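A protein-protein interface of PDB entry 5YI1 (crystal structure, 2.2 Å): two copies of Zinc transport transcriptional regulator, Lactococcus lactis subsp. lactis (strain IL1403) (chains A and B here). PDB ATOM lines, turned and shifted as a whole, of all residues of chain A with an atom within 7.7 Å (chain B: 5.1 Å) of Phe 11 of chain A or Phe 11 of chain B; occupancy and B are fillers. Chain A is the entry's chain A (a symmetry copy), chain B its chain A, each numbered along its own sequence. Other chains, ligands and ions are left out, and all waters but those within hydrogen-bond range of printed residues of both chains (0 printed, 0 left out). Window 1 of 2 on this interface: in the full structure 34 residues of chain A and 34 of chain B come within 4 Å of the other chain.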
ATOM      1  N   MET A   2      17.972 -46.321 -24.218  1.00  0.00           N
ATOM      2  CA  MET A   2      19.059 -45.359 -23.981  1.00  0.00           C
ATOM      3  C   MET A   2      18.856 -44.517 -22.720  1.00  0.00           C
ATOM      4  O   MET A   2      17.792 -43.918 -22.519  1.00  0.00           O
ATOM      5  CB  MET A   2      19.268 -44.449 -25.195  1.00  0.00           C
ATOM      6  CG  MET A   2      20.315 -43.358 -24.973  1.00  0.00           C
ATOM      7  SD  MET A   2      20.696 -42.374 -26.440  1.00  0.00           S
ATOM      8  CE  MET A   2      19.085 -42.215 -27.227  1.00  0.00           C
ATOM      9  N   LEU A   4      19.148 -41.476 -20.032  1.00  0.00           N
ATOM     10  CA  LEU A   4      18.942 -40.052 -20.245  1.00  0.00           C
ATOM     11  C   LEU A   4      20.304 -39.391 -20.394  1.00  0.00           C
ATOM     12  O   LEU A   4      20.489 -38.508 -21.228  1.00  0.00           O
ATOM     13  CB  LEU A   4      18.165 -39.433 -19.082  1.00  0.00           C
ATOM     14  CG  LEU A   4      17.805 -37.964 -19.293  1.00  0.00           C
ATOM     15  CD1 LEU A   4      16.790 -37.841 -20.432  1.00  0.00           C
ATOM     16  CD2 LEU A   4      17.289 -37.313 -18.013  1.00  0.00           C
ATOM     17  N   ALA A   5      21.259 -39.836 -19.586  1.00  0.00           N
ATOM     18  CA  ALA A   5      22.637 -39.346 -19.686  1.00  0.00           C
ATOM     19  C   ALA A   5      23.148 -39.437 -21.123  1.00  0.00           C
ATOM     20  O   ALA A   5      23.676 -38.462 -21.674  1.00  0.00           O
ATOM     21  CB  ALA A   5      23.548 -40.118 -18.746  1.00  0.00           C
ATOM     22  N   ASN A   6      22.983 -40.608 -21.729  1.00  0.00           N
ATOM     23  CA  ASN A   6      23.383 -40.797 -23.117  1.00  0.00           C
ATOM     24  C   ASN A   6      22.570 -39.947 -24.089  1.00  0.00           C
ATOM     25  O   ASN A   6      23.098 -39.484 -25.099  1.00  0.00           O
ATOM     26  CB  ASN A   6      23.315 -42.271 -23.513  1.00  0.00           C
ATOM     27  CG  ASN A   6      24.513 -43.059 -23.020  1.00  0.00           C
ATOM     28  OD1 ASN A   6      25.638 -42.578 -23.066  1.00  0.00           O
ATOM     29  ND2 ASN A   6      24.273 -44.267 -22.530  1.00  0.00           N
ATOM     30  N   GLN A   7      21.287 -39.746 -23.792  1.00  0.00           N
ATOM     31  CA  GLN A   7      20.466 -38.904 -24.651  1.00  0.00           C
ATOM     32  C   GLN A   7      20.988 -37.471 -24.587  1.00  0.00           C
ATOM     33  O   GLN A   7      21.114 -36.783 -25.602  1.00  0.00           O
ATOM     34  CB  GLN A   7      18.995 -38.946 -24.228  1.00  0.00           C
ATOM     35  CG  GLN A   7      18.341 -40.338 -24.233  1.00  0.00           C
ATOM     36  CD  GLN A   7      16.848 -40.271 -23.867  1.00  0.00           C
ATOM     37  OE1 GLN A   7      16.185 -39.254 -24.104  1.00  0.00           O
ATOM     38  NE2 GLN A   7      16.326 -41.350 -23.295  1.00  0.00           N
ATOM     39  N   ILE A   8      21.281 -37.020 -23.378  1.00  0.00           N
ATOM     40  CA  ILE A   8      21.817 -35.683 -23.202  1.00  0.00           C
ATOM     41  C   ILE A   8      23.171 -35.552 -23.920  1.00  0.00           C
ATOM     42  O   ILE A   8      23.433 -34.569 -24.633  1.00  0.00           O
ATOM     43  CB  ILE A   8      21.964 -35.343 -21.701  1.00  0.00           C
ATOM     44  CG1 ILE A   8      20.572 -35.193 -21.051  1.00  0.00           C
ATOM     45  CG2 ILE A   8      22.822 -34.093 -21.526  1.00  0.00           C
ATOM     46  CD1 ILE A   8      20.560 -35.422 -19.529  1.00  0.00           C
ATOM     47  N   ASP A   9      24.024 -36.551 -23.743  1.00  0.00           N
ATOM     48  CA  ASP A   9      25.336 -36.521 -24.401  1.00  0.00           C
ATOM     49  C   ASP A   9      25.171 -36.379 -25.923  1.00  0.00           C
ATOM     50  O   ASP A   9      25.751 -35.493 -26.534  1.00  0.00           O
ATOM     51  CB  ASP A   9      26.153 -37.766 -24.026  1.00  0.00           C
ATOM     52  CG  ASP A   9      27.557 -37.766 -24.638  1.00  0.00           C
ATOM     53  OD1 ASP A   9      28.307 -36.784 -24.448  1.00  0.00           O
ATOM     54  OD2 ASP A   9      27.903 -38.763 -25.307  1.00  0.00           O
ATOM     55  N   GLN A  10      24.340 -37.228 -26.518  1.00  0.00           N
ATOM     56  CA  GLN A  10      24.087 -37.197 -27.960  1.00  0.00           C
ATOM     57  C   GLN A  10      23.453 -35.897 -28.423  1.00  0.00           C
ATOM     58  O   GLN A  10      23.753 -35.398 -29.517  1.00  0.00           O
ATOM     59  CB  GLN A  10      23.194 -38.374 -28.371  1.00  0.00           C
ATOM     60  CG  GLN A  10      23.909 -39.726 -28.321  1.00  0.00           C
ATOM     61  CD  GLN A  10      23.339 -40.737 -29.305  1.00  0.00           C
ATOM     62  OE1 GLN A  10      23.149 -41.911 -28.970  1.00  0.00           O
ATOM     63  NE2 GLN A  10      23.073 -40.288 -30.528  1.00  0.00           N
ATOM     64  N   PHE A  11      22.550 -35.359 -27.604  1.00  0.00           N
ATOM     65  CA  PHE A  11      21.922 -34.092 -27.936  1.00  0.00           C
ATOM     66  C   PHE A  11      22.934 -32.964 -27.985  1.00  0.00           C
ATOM     67  O   PHE A  11      22.922 -32.164 -28.910  1.00  0.00           O
ATOM     68  CB  PHE A  11      20.821 -33.721 -26.941  1.00  0.00           C
ATOM     69  CG  PHE A  11      20.473 -32.259 -26.962  1.00  0.00           C
ATOM     70  CD1 PHE A  11      19.680 -31.739 -27.964  1.00  0.00           C
ATOM     71  CD2 PHE A  11      20.955 -31.404 -25.985  1.00  0.00           C
ATOM     72  CE1 PHE A  11      19.366 -30.391 -27.989  1.00  0.00           C
ATOM     73  CE2 PHE A  11      20.642 -30.068 -26.001  1.00  0.00           C
ATOM     74  CZ  PHE A  11      19.842 -29.555 -27.005  1.00  0.00           C
ATOM     75  N   LEU A  12      23.792 -32.889 -26.976  1.00  0.00           N
ATOM     76  CA  LEU A  12      24.790 -31.821 -26.930  1.00  0.00           C
ATOM     77  C   LEU A  12      25.807 -31.978 -28.063  1.00  0.00           C
ATOM     78  O   LEU A  12      26.301 -30.990 -28.599  1.00  0.00           O
ATOM     79  CB  LEU A  12      25.490 -31.788 -25.567  1.00  0.00           C
ATOM     80  CG  LEU A  12      24.614 -31.361 -24.383  1.00  0.00           C
ATOM     81  CD1 LEU A  12      25.278 -31.718 -23.062  1.00  0.00           C
ATOM     82  CD2 LEU A  12      24.306 -29.876 -24.468  1.00  0.00           C
ATOM     83  N   GLY A  13      26.117 -33.221 -28.420  1.00  0.00           N
ATOM     84  CA  GLY A  13      27.010 -33.487 -29.537  1.00  0.00           C
ATOM     85  C   GLY A  13      26.463 -32.962 -30.852  1.00  0.00           C
ATOM     86  O   GLY A  13      27.200 -32.428 -31.668  1.00  0.00           O
ATOM     87  N   THR A  14      25.155 -33.105 -31.041  1.00  0.00           N
ATOM     88  CA  THR A  14      24.467 -32.610 -32.234  1.00  0.00           C
ATOM     89  C   THR A  14      24.478 -31.085 -32.295  1.00  0.00           C
ATOM     90  O   THR A  14      24.702 -30.498 -33.356  1.00  0.00           O
ATOM     91  CB  THR A  14      23.009 -33.131 -32.287  1.00  0.00           C
ATOM     92  OG1 THR A  14      23.020 -34.562 -32.242  1.00  0.00           O
ATOM     93  CG2 THR A  14      22.293 -32.661 -33.550  1.00  0.00           C
ATOM     94  N   ILE A  15      24.251 -30.436 -31.160  1.00  0.00           N
ATOM     95  CA  ILE A  15      24.282 -28.976 -31.144  1.00  0.00           C
ATOM     96  C   ILE A  15      25.711 -28.444 -31.364  1.00  0.00           C
ATOM     97  O   ILE A  15      25.908 -27.401 -31.980  1.00  0.00           O
ATOM     98  CB  ILE A  15      23.665 -28.384 -29.842  1.00  0.00           C
ATOM     99  CG1 ILE A  15      22.223 -28.878 -29.641  1.00  0.00           C
ATOM    100  CG2 ILE A  15      23.696 -26.864 -29.872  1.00  0.00           C
ATOM    101  CD1 ILE A  15      21.281 -28.524 -30.766  1.00  0.00           C
ATOM    102  N   MET A  16      26.701 -29.169 -30.855  1.00  0.00           N
ATOM    103  CA  MET A  16      28.099 -28.785 -31.017  1.00  0.00           C
ATOM    104  C   MET A  16      28.616 -29.035 -32.443  1.00  0.00           C
ATOM    105  O   MET A  16      29.387 -28.245 -32.977  1.00  0.00           O
ATOM    106  CB  MET A  16      28.977 -29.502 -29.990  1.00  0.00           C
ATOM    107  CG  MET A  16      28.963 -28.863 -28.607  1.00  0.00           C
ATOM    108  SD  MET A  16      29.947 -29.821 -27.428  1.00  0.00           S
ATOM    109  CE  MET A  16      29.447 -29.075 -25.872  1.00  0.00           C
ATOM    110  N   GLN A  17      28.194 -30.138 -33.049  1.00  0.00           N
ATOM    111  CA  GLN A  17      28.468 -30.381 -34.460  1.00  0.00           C
ATOM    112  C   GLN A  17      27.883 -29.256 -35.322  1.00  0.00           C
ATOM    113  O   GLN A  17      28.595 -28.651 -36.128  1.00  0.00           O
ATOM    114  CB  GLN A  17      27.892 -31.732 -34.887  1.00  0.00           C
ATOM    115  CG  GLN A  17      28.285 -32.174 -36.290  1.00  0.00           C
ATOM    116  CD  GLN A  17      28.916 -33.562 -36.306  1.00  0.00           C
ATOM    117  OE1 GLN A  17      29.754 -33.888 -35.460  1.00  0.00           O
ATOM    118  NE2 GLN A  17      28.507 -34.388 -37.268  1.00  0.00           N
ATOM    119  N   TYR A 119      11.187 -22.398 -31.253  1.00  0.00           N
ATOM    120  CA  TYR A 119      11.292 -22.770 -29.845  1.00  0.00           C
ATOM    121  C   TYR A 119       9.936 -22.617 -29.138  1.00  0.00           C
ATOM    122  O   TYR A 119       9.525 -23.480 -28.353  1.00  0.00           O
ATOM    123  CB  TYR A 119      12.367 -21.944 -29.136  1.00  0.00           C
ATOM    124  CG  TYR A 119      13.724 -22.042 -29.798  1.00  0.00           C
ATOM    125  CD1 TYR A 119      14.049 -23.146 -30.585  1.00  0.00           C
ATOM    126  CD2 TYR A 119      14.682 -21.038 -29.642  1.00  0.00           C
ATOM    127  CE1 TYR A 119      15.278 -23.250 -31.199  1.00  0.00           C
ATOM    128  CE2 TYR A 119      15.919 -21.132 -30.258  1.00  0.00           C
ATOM    129  CZ  TYR A 119      16.211 -22.241 -31.041  1.00  0.00           C
ATOM    130  OH  TYR A 119      17.435 -22.370 -31.662  1.00  0.00           O
ATOM    131  N   PHE A 137      15.723 -28.038 -15.879  1.00  0.00           N
ATOM    132  CA  PHE A 137      16.720 -28.916 -16.464  1.00  0.00           C
ATOM    133  C   PHE A 137      17.751 -28.081 -17.219  1.00  0.00           C
ATOM    134  O   PHE A 137      18.957 -28.223 -17.013  1.00  0.00           O
ATOM    135  CB  PHE A 137      16.059 -29.933 -17.398  1.00  0.00           C
ATOM    136  CG  PHE A 137      17.036 -30.699 -18.223  1.00  0.00           C
ATOM    137  CD1 PHE A 137      17.780 -31.720 -17.656  1.00  0.00           C
ATOM    138  CD2 PHE A 137      17.254 -30.366 -19.558  1.00  0.00           C
ATOM    139  CE1 PHE A 137      18.712 -32.433 -18.418  1.00  0.00           C
ATOM    140  CE2 PHE A 137      18.159 -31.071 -20.317  1.00  0.00           C
ATOM    141  CZ  PHE A 137      18.897 -32.110 -19.737  1.00  0.00           C
ATOM    142  N   LEU A 138      17.263 -27.205 -18.094  1.00  0.00           N
ATOM    143  CA  LEU A 138      18.144 -26.379 -18.920  1.00  0.00           C
ATOM    144  C   LEU A 138      19.020 -25.442 -18.085  1.00  0.00           C
ATOM    145  O   LEU A 138      20.196 -25.270 -18.394  1.00  0.00           O
ATOM    146  CB  LEU A 138      17.353 -25.583 -19.966  1.00  0.00           C
ATOM    147  CG  LEU A 138      16.666 -26.326 -21.127  1.00  0.00           C
ATOM    148  CD1 LEU A 138      15.972 -25.352 -22.060  1.00  0.00           C
ATOM    149  CD2 LEU A 138      17.632 -27.199 -21.895  1.00  0.00           C
ATOM    150  N   SER A 139      18.471 -24.837 -17.029  1.00  0.00           N
ATOM    151  CA  SER A 139      19.298 -23.959 -16.190  1.00  0.00           C
ATOM    152  C   SER A 139      20.449 -24.743 -15.571  1.00  0.00           C
ATOM    153  O   SER A 139      21.581 -24.294 -15.585  1.00  0.00           O
ATOM    154  CB  SER A 139      18.490 -23.299 -15.071  1.00  0.00           C
ATOM    155  OG  SER A 139      17.320 -22.716 -15.596  1.00  0.00           O
ATOM    156  N   ALA A 140      20.145 -25.912 -15.012  1.00  0.00           N
ATOM    157  CA  ALA A 140      21.171 -26.702 -14.340  1.00  0.00           C
ATOM    158  C   ALA A 140      22.230 -27.177 -15.325  1.00  0.00           C
ATOM    159  O   ALA A 140      23.410 -27.194 -15.012  1.00  0.00           O
ATOM    160  CB  ALA A 140      20.552 -27.895 -13.578  1.00  0.00           C
ATOM    161  N   LEU A 141      21.808 -27.559 -16.523  1.00  0.00           N
ATOM    162  CA  LEU A 141      22.755 -27.991 -17.540  1.00  0.00           C
ATOM    163  C   LEU A 141      23.595 -26.796 -18.063  1.00  0.00           C
ATOM    164  O   LEU A 141      24.802 -26.911 -18.285  1.00  0.00           O
ATOM    165  CB  LEU A 141      22.027 -28.678 -18.696  1.00  0.00           C
ATOM    166  CG  LEU A 141      22.874 -29.310 -19.807  1.00  0.00           C
ATOM    167  CD1 LEU A 141      23.917 -30.278 -19.244  1.00  0.00           C
ATOM    168  CD2 LEU A 141      21.980 -30.006 -20.801  1.00  0.00           C
ATOM    169  N   THR A 142      22.956 -25.650 -18.258  1.00  0.00           N
ATOM    170  CA  THR A 142      23.693 -24.431 -18.619  1.00  0.00           C
ATOM    171  C   THR A 142      24.912 -24.232 -17.707  1.00  0.00           C
ATOM    172  O   THR A 142      26.026 -24.053 -18.175  1.00  0.00           O
ATOM    173  CB  THR A 142      22.805 -23.175 -18.512  1.00  0.00           C
ATOM    174  OG1 THR A 142      21.710 -23.274 -19.428  1.00  0.00           O
ATOM    175  CG2 THR A 142      23.621 -21.929 -18.832  1.00  0.00           C
ATOM    176  N   GLU A 143      24.684 -24.286 -16.400  1.00  0.00           N
ATOM    177  CA  GLU A 143      25.746 -24.099 -15.428  1.00  0.00           C
ATOM    178  C   GLU A 143      26.978 -24.943 -15.747  1.00  0.00           C
ATOM    179  O   GLU A 143      28.113 -24.459 -15.657  1.00  0.00           O
ATOM    180  CB  GLU A 143      25.240 -24.423 -14.029  1.00  0.00           C
ATOM    181  CG  GLU A 143      24.216 -23.453 -13.491  1.00  0.00           C
ATOM    182  CD  GLU A 143      23.811 -23.802 -12.068  1.00  0.00           C
ATOM    183  OE1 GLU A 143      24.606 -24.466 -11.365  1.00  0.00           O
ATOM    184  OE2 GLU A 143      22.695 -23.426 -11.657  1.00  0.00           O
ATOM    185  N   PHE A 145      28.243 -25.590 -18.305  1.00  0.00           N
ATOM    186  CA  PHE A 145      28.953 -25.020 -19.456  1.00  0.00           C
ATOM    187  C   PHE A 145      29.282 -23.521 -19.312  1.00  0.00           C
ATOM    188  O   PHE A 145      29.661 -22.868 -20.286  1.00  0.00           O
ATOM    189  CB  PHE A 145      28.172 -25.274 -20.752  1.00  0.00           C
ATOM    190  CG  PHE A 145      28.091 -26.726 -21.122  1.00  0.00           C
ATOM    191  CD1 PHE A 145      29.078 -27.312 -21.903  1.00  0.00           C
ATOM    192  CD2 PHE A 145      27.043 -27.519 -20.665  1.00  0.00           C
ATOM    193  CE1 PHE A 145      29.019 -28.652 -22.227  1.00  0.00           C
ATOM    194  CE2 PHE A 145      26.978 -28.864 -20.990  1.00  0.00           C
ATOM    195  CZ  PHE A 145      27.967 -29.432 -21.772  1.00  0.00           C
ATOM    196  N   ASN B   6      12.923 -18.006 -25.164  1.00  0.00           N
ATOM    197  CA  ASN B   6      14.144 -17.263 -24.883  1.00  0.00           C
ATOM    198  C   ASN B   6      15.136 -18.052 -24.033  1.00  0.00           C
ATOM    199  O   ASN B   6      16.346 -17.922 -24.211  1.00  0.00           O
ATOM    200  CB  ASN B   6      13.833 -15.918 -24.228  1.00  0.00           C
ATOM    201  CG  ASN B   6      13.383 -14.875 -25.232  1.00  0.00           C
ATOM    202  OD1 ASN B   6      13.927 -14.787 -26.326  1.00  0.00           O
ATOM    203  ND2 ASN B   6      12.377 -14.092 -24.871  1.00  0.00           N
ATOM    204  N   GLN B   7      14.629 -18.864 -23.107  1.00  0.00           N
ATOM    205  CA  GLN B   7      15.516 -19.683 -22.294  1.00  0.00           C
ATOM    206  C   GLN B   7      16.216 -20.699 -23.193  1.00  0.00           C
ATOM    207  O   GLN B   7      17.422 -20.932 -23.088  1.00  0.00           O
ATOM    208  CB  GLN B   7      14.746 -20.406 -21.186  1.00  0.00           C
ATOM    209  CG  GLN B   7      13.978 -19.499 -20.210  1.00  0.00           C
ATOM    210  CD  GLN B   7      13.297 -20.308 -19.091  1.00  0.00           C
ATOM    211  OE1 GLN B   7      13.767 -21.392 -18.721  1.00  0.00           O
ATOM    212  NE2 GLN B   7      12.202 -19.781 -18.558  1.00  0.00           N
ATOM    213  N   ILE B   8      15.445 -21.314 -24.075  1.00  0.00           N
ATOM    214  CA  ILE B   8      16.011 -22.275 -25.003  1.00  0.00           C
ATOM    215  C   ILE B   8      17.043 -21.591 -25.916  1.00  0.00           C
ATOM    216  O   ILE B   8      18.151 -22.106 -26.139  1.00  0.00           O
ATOM    217  CB  ILE B   8      14.900 -22.943 -25.846  1.00  0.00           C
ATOM    218  CG1 ILE B   8      14.038 -23.863 -24.956  1.00  0.00           C
ATOM    219  CG2 ILE B   8      15.514 -23.691 -27.027  1.00  0.00           C
ATOM    220  CD1 ILE B   8      12.622 -24.121 -25.503  1.00  0.00           C
ATOM    221  N   ASP B   9      16.684 -20.423 -26.430  1.00  0.00           N
ATOM    222  CA  ASP B   9      17.611 -19.689 -27.301  1.00  0.00           C
ATOM    223  C   ASP B   9      18.942 -19.434 -26.577  1.00  0.00           C
ATOM    224  O   ASP B   9      20.003 -19.759 -27.087  1.00  0.00           O
ATOM    225  CB  ASP B   9      16.966 -18.385 -27.794  1.00  0.00           C
ATOM    226  CG  ASP B   9      17.863 -17.601 -28.754  1.00  0.00           C
ATOM    227  OD1 ASP B   9      18.321 -18.171 -29.769  1.00  0.00           O
ATOM    228  OD2 ASP B   9      18.102 -16.404 -28.485  1.00  0.00           O
ATOM    229  N   GLN B  10      18.870 -18.892 -25.364  1.00  0.00           N
ATOM    230  CA  GLN B  10      20.061 -18.603 -24.564  1.00  0.00           C
ATOM    231  C   GLN B  10      20.854 -19.849 -24.209  1.00  0.00           C
ATOM    232  O   GLN B  10      22.093 -19.822 -24.166  1.00  0.00           O
ATOM    233  CB  GLN B  10      19.674 -17.864 -23.278  1.00  0.00           C
ATOM    234  CG  GLN B  10      19.236 -16.417 -23.517  1.00  0.00           C
ATOM    235  CD  GLN B  10      19.500 -15.510 -22.323  1.00  0.00           C
ATOM    236  OE1 GLN B  10      18.654 -14.690 -21.951  1.00  0.00           O
ATOM    237  NE2 GLN B  10      20.678 -15.648 -21.724  1.00  0.00           N
ATOM    238  N   PHE B  11      20.142 -20.939 -23.924  1.00  0.00           N
ATOM    239  CA  PHE B  11      20.809 -22.192 -23.619  1.00  0.00           C
ATOM    240  C   PHE B  11      21.605 -22.703 -24.804  1.00  0.00           C
ATOM    241  O   PHE B  11      22.745 -23.118 -24.650  1.00  0.00           O
ATOM    242  CB  PHE B  11      19.821 -23.276 -23.187  1.00  0.00           C
ATOM    243  CG  PHE B  11      20.377 -24.667 -23.309  1.00  0.00           C
ATOM    244  CD1 PHE B  11      21.258 -25.157 -22.366  1.00  0.00           C
ATOM    245  CD2 PHE B  11      20.030 -25.477 -24.377  1.00  0.00           C
ATOM    246  CE1 PHE B  11      21.778 -26.435 -22.482  1.00  0.00           C
ATOM    247  CE2 PHE B  11      20.538 -26.746 -24.494  1.00  0.00           C
ATOM    248  CZ  PHE B  11      21.415 -27.233 -23.542  1.00  0.00           C
ATOM    249  N   LEU B  12      20.993 -22.694 -25.981  1.00  0.00           N
ATOM    250  CA  LEU B  12      21.675 -23.189 -27.176  1.00  0.00           C
ATOM    251  C   LEU B  12      22.854 -22.282 -27.543  1.00  0.00           C
ATOM    252  O   LEU B  12      23.873 -22.754 -28.040  1.00  0.00           O
ATOM    253  CB  LEU B  12      20.698 -23.316 -28.350  1.00  0.00           C
ATOM    254  CG  LEU B  12      19.630 -24.407 -28.205  1.00  0.00           C
ATOM    255  CD1 LEU B  12      18.511 -24.205 -29.215  1.00  0.00           C
ATOM    256  CD2 LEU B  12      20.262 -25.781 -28.342  1.00  0.00           C
ATOM    257  N   GLY B  13      22.708 -20.984 -27.298  1.00  0.00           N
ATOM    258  CA  GLY B  13      23.792 -20.043 -27.531  1.00  0.00           C
ATOM    259  C   GLY B  13      25.009 -20.339 -26.674  1.00  0.00           C
ATOM    260  O   GLY B  13      26.138 -20.236 -27.133  1.00  0.00           O
ATOM    261  N   THR B  14      24.766 -20.725 -25.426  1.00  0.00           N
ATOM    262  CA  THR B  14      25.828 -21.093 -24.488  1.00  0.00           C
ATOM    263  C   THR B  14      26.541 -22.371 -24.922  1.00  0.00           C
ATOM    264  O   THR B  14      27.769 -22.462 -24.853  1.00  0.00           O
ATOM    265  CB  THR B  14      25.265 -21.262 -23.055  1.00  0.00           C
ATOM    266  OG1 THR B  14      24.612 -20.050 -22.661  1.00  0.00           O
ATOM    267  CG2 THR B  14      26.369 -21.599 -22.057  1.00  0.00           C
ATOM    268  N   ILE B  15      25.782 -23.357 -25.383  1.00  0.00           N
ATOM    269  CA  ILE B  15      26.405 -24.594 -25.846  1.00  0.00           C
ATOM    270  C   ILE B  15      27.201 -24.365 -27.145  1.00  0.00           C
ATOM    271  O   ILE B  15      28.234 -24.989 -27.370  1.00  0.00           O
ATOM    272  CB  ILE B  15      25.375 -25.747 -26.023  1.00  0.00           C
ATOM    273  CG1 ILE B  15      24.608 -26.007 -24.715  1.00  0.00           C
ATOM    274  CG2 ILE B  15      26.064 -27.022 -26.484  1.00  0.00           C
ATOM    275  CD1 ILE B  15      25.484 -26.384 -23.545  1.00  0.00           C
ATOM    276  N   LEU B 138      14.059 -32.973 -25.667  1.00  0.00           N
ATOM    277  CA  LEU B 138      15.359 -33.054 -26.331  1.00  0.00           C
ATOM    278  C   LEU B 138      15.273 -33.722 -27.706  1.00  0.00           C
ATOM    279  O   LEU B 138      15.924 -33.270 -28.645  1.00  0.00           O
ATOM    280  CB  LEU B 138      16.397 -33.766 -25.454  1.00  0.00           C
ATOM    281  CG  LEU B 138      16.897 -33.087 -24.165  1.00  0.00           C
ATOM    282  CD1 LEU B 138      17.940 -33.942 -23.471  1.00  0.00           C
ATOM    283  CD2 LEU B 138      17.438 -31.699 -24.427  1.00  0.00           C
ATOM    284  N   LEU B 141      13.747 -31.174 -30.129  1.00  0.00           N
ATOM    285  CA  LEU B 141      14.688 -30.097 -30.402  1.00  0.00           C
ATOM    286  C   LEU B 141      15.875 -30.601 -31.265  1.00  0.00           C
ATOM    287  O   LEU B 141      16.335 -29.917 -32.181  1.00  0.00           O
ATOM    288  CB  LEU B 141      15.197 -29.485 -29.098  1.00  0.00           C
ATOM    289  CG  LEU B 141      16.107 -28.254 -29.186  1.00  0.00           C
ATOM    290  CD1 LEU B 141      15.478 -27.144 -30.032  1.00  0.00           C
ATOM    291  CD2 LEU B 141      16.429 -27.753 -27.802  1.00  0.00           C
ATOM    292  N   THR B 142      16.370 -31.796 -30.970  1.00  0.00           N
ATOM    293  CA  THR B 142      17.401 -32.412 -31.817  1.00  0.00           C
ATOM    294  C   THR B 142      17.020 -32.325 -33.302  1.00  0.00           C
ATOM    295  O   THR B 142      17.795 -31.859 -34.125  1.00  0.00           O
ATOM    296  CB  THR B 142      17.616 -33.898 -31.465  1.00  0.00           C
ATOM    297  OG1 THR B 142      18.076 -34.015 -30.115  1.00  0.00           O
ATOM    298  CG2 THR B 142      18.644 -34.514 -32.405  1.00  0.00           C
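The side-chain hydroxyl (OG1) of Thr 14 of chain B sits at hydrogen-bond distance from the backbone carbonyl oxygen (O) of Gln 10 of chain B (2.9 Å).
O of Leu 138 of chain B sits at hydrogen-bond distance from OG1 of Thr 142 of chain B, 2.7 Å away.
OG1 of Thr 142 of chain A is in hydrogen-bond range of O of Leu 138 of chain A (2.7 Å).
Printed residues of chain B within 4 Å of Tyr 119 of chain A: Ile 8, Asp 9 and Leu 12.
Of chain A, only Phe 11, Leu 138, Leu 141 and Thr 142 come within 4 Å of Phe 11 of chain B.
Of the printed residues of chain A, Leu 141 of chain B touches Phe 11 (3.9 Å).
The nearest residue of chain B that does not touch Phe 11 of chain A is Leu 12 of chain B (4.03 Å).
Among the printed residues, pairs that only touch across the chains: Tyr 119 of chain A with Leu 12 of chain B (3.2 Å), Phe 145 of chain A with Ile 15 of chain B (3.5 Å), Phe 11 of chain A with Thr 142 of chain B (3.5 Å), Thr 142 of chain A with Phe 11 of chain B (3.5 Å), Phe 11 of chain A with Phe 11 of chain B (3.6 Å), Tyr 119 of chain A with Ile 8 of chain B (3.7 Å), Tyr 119 of chain A with Asp 9 of chain B (3.7 Å), Leu 138 of chain A with Ile 8 of chain B (3.8 Å), Ile 8 of chain A with Leu 138 of chain B (3.8 Å), Leu 12 of chain A with Ile 15 of chain B (3.8 Å), Ile 15 of chain A with Leu 12 of chain B (3.8 Å), Leu 138 of chain A with Phe 11 of chain B (3.9 Å), Phe 11 of chain A with Leu 138 of chain B (3.9 Å), Leu 141 of chain A with Phe 11 of chain B (3.9 Å), Phe 11 of chain A with Leu 141 of chain B (3.9 Å) and Phe 145 of chain A with Thr 14 of chain B (3.9 Å).
Phe 11 of chain B touches its own counterpart, Phe 11 of chain A.
Phe 11 of chain A touches Leu 138 of chain B, and with the chains exchanged Leu 138 of chain A touches Phe 11 of chain B.
Phe 11 of chain A touches Leu 141 of chain B, and with the chains exchanged Leu 141 of chain A touches Phe 11 of chain B.
Leu 12 of chain A touches Ile 15 of chain B, and with the chains exchanged Ile 15 of chain A touches Leu 12 of chain B.
13 positions are printed for both chains.
Hydrophobic or aromatic side chains of chain A within 4 Å of the printed part of chain B: Ile 8, Phe 11, Leu 12, Ile 15, Tyr 119, Leu 138, Leu 141 and Phe 145.
Hydrophobic or aromatic side chains of chain B within 4 Å of the printed part of chain A: Ile 8, Phe 11, Leu 12, Ile 15, Leu 138 and Leu 141.
Along chain B the printed residues that touch a printed residue of chain A span positions 8 to 142.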
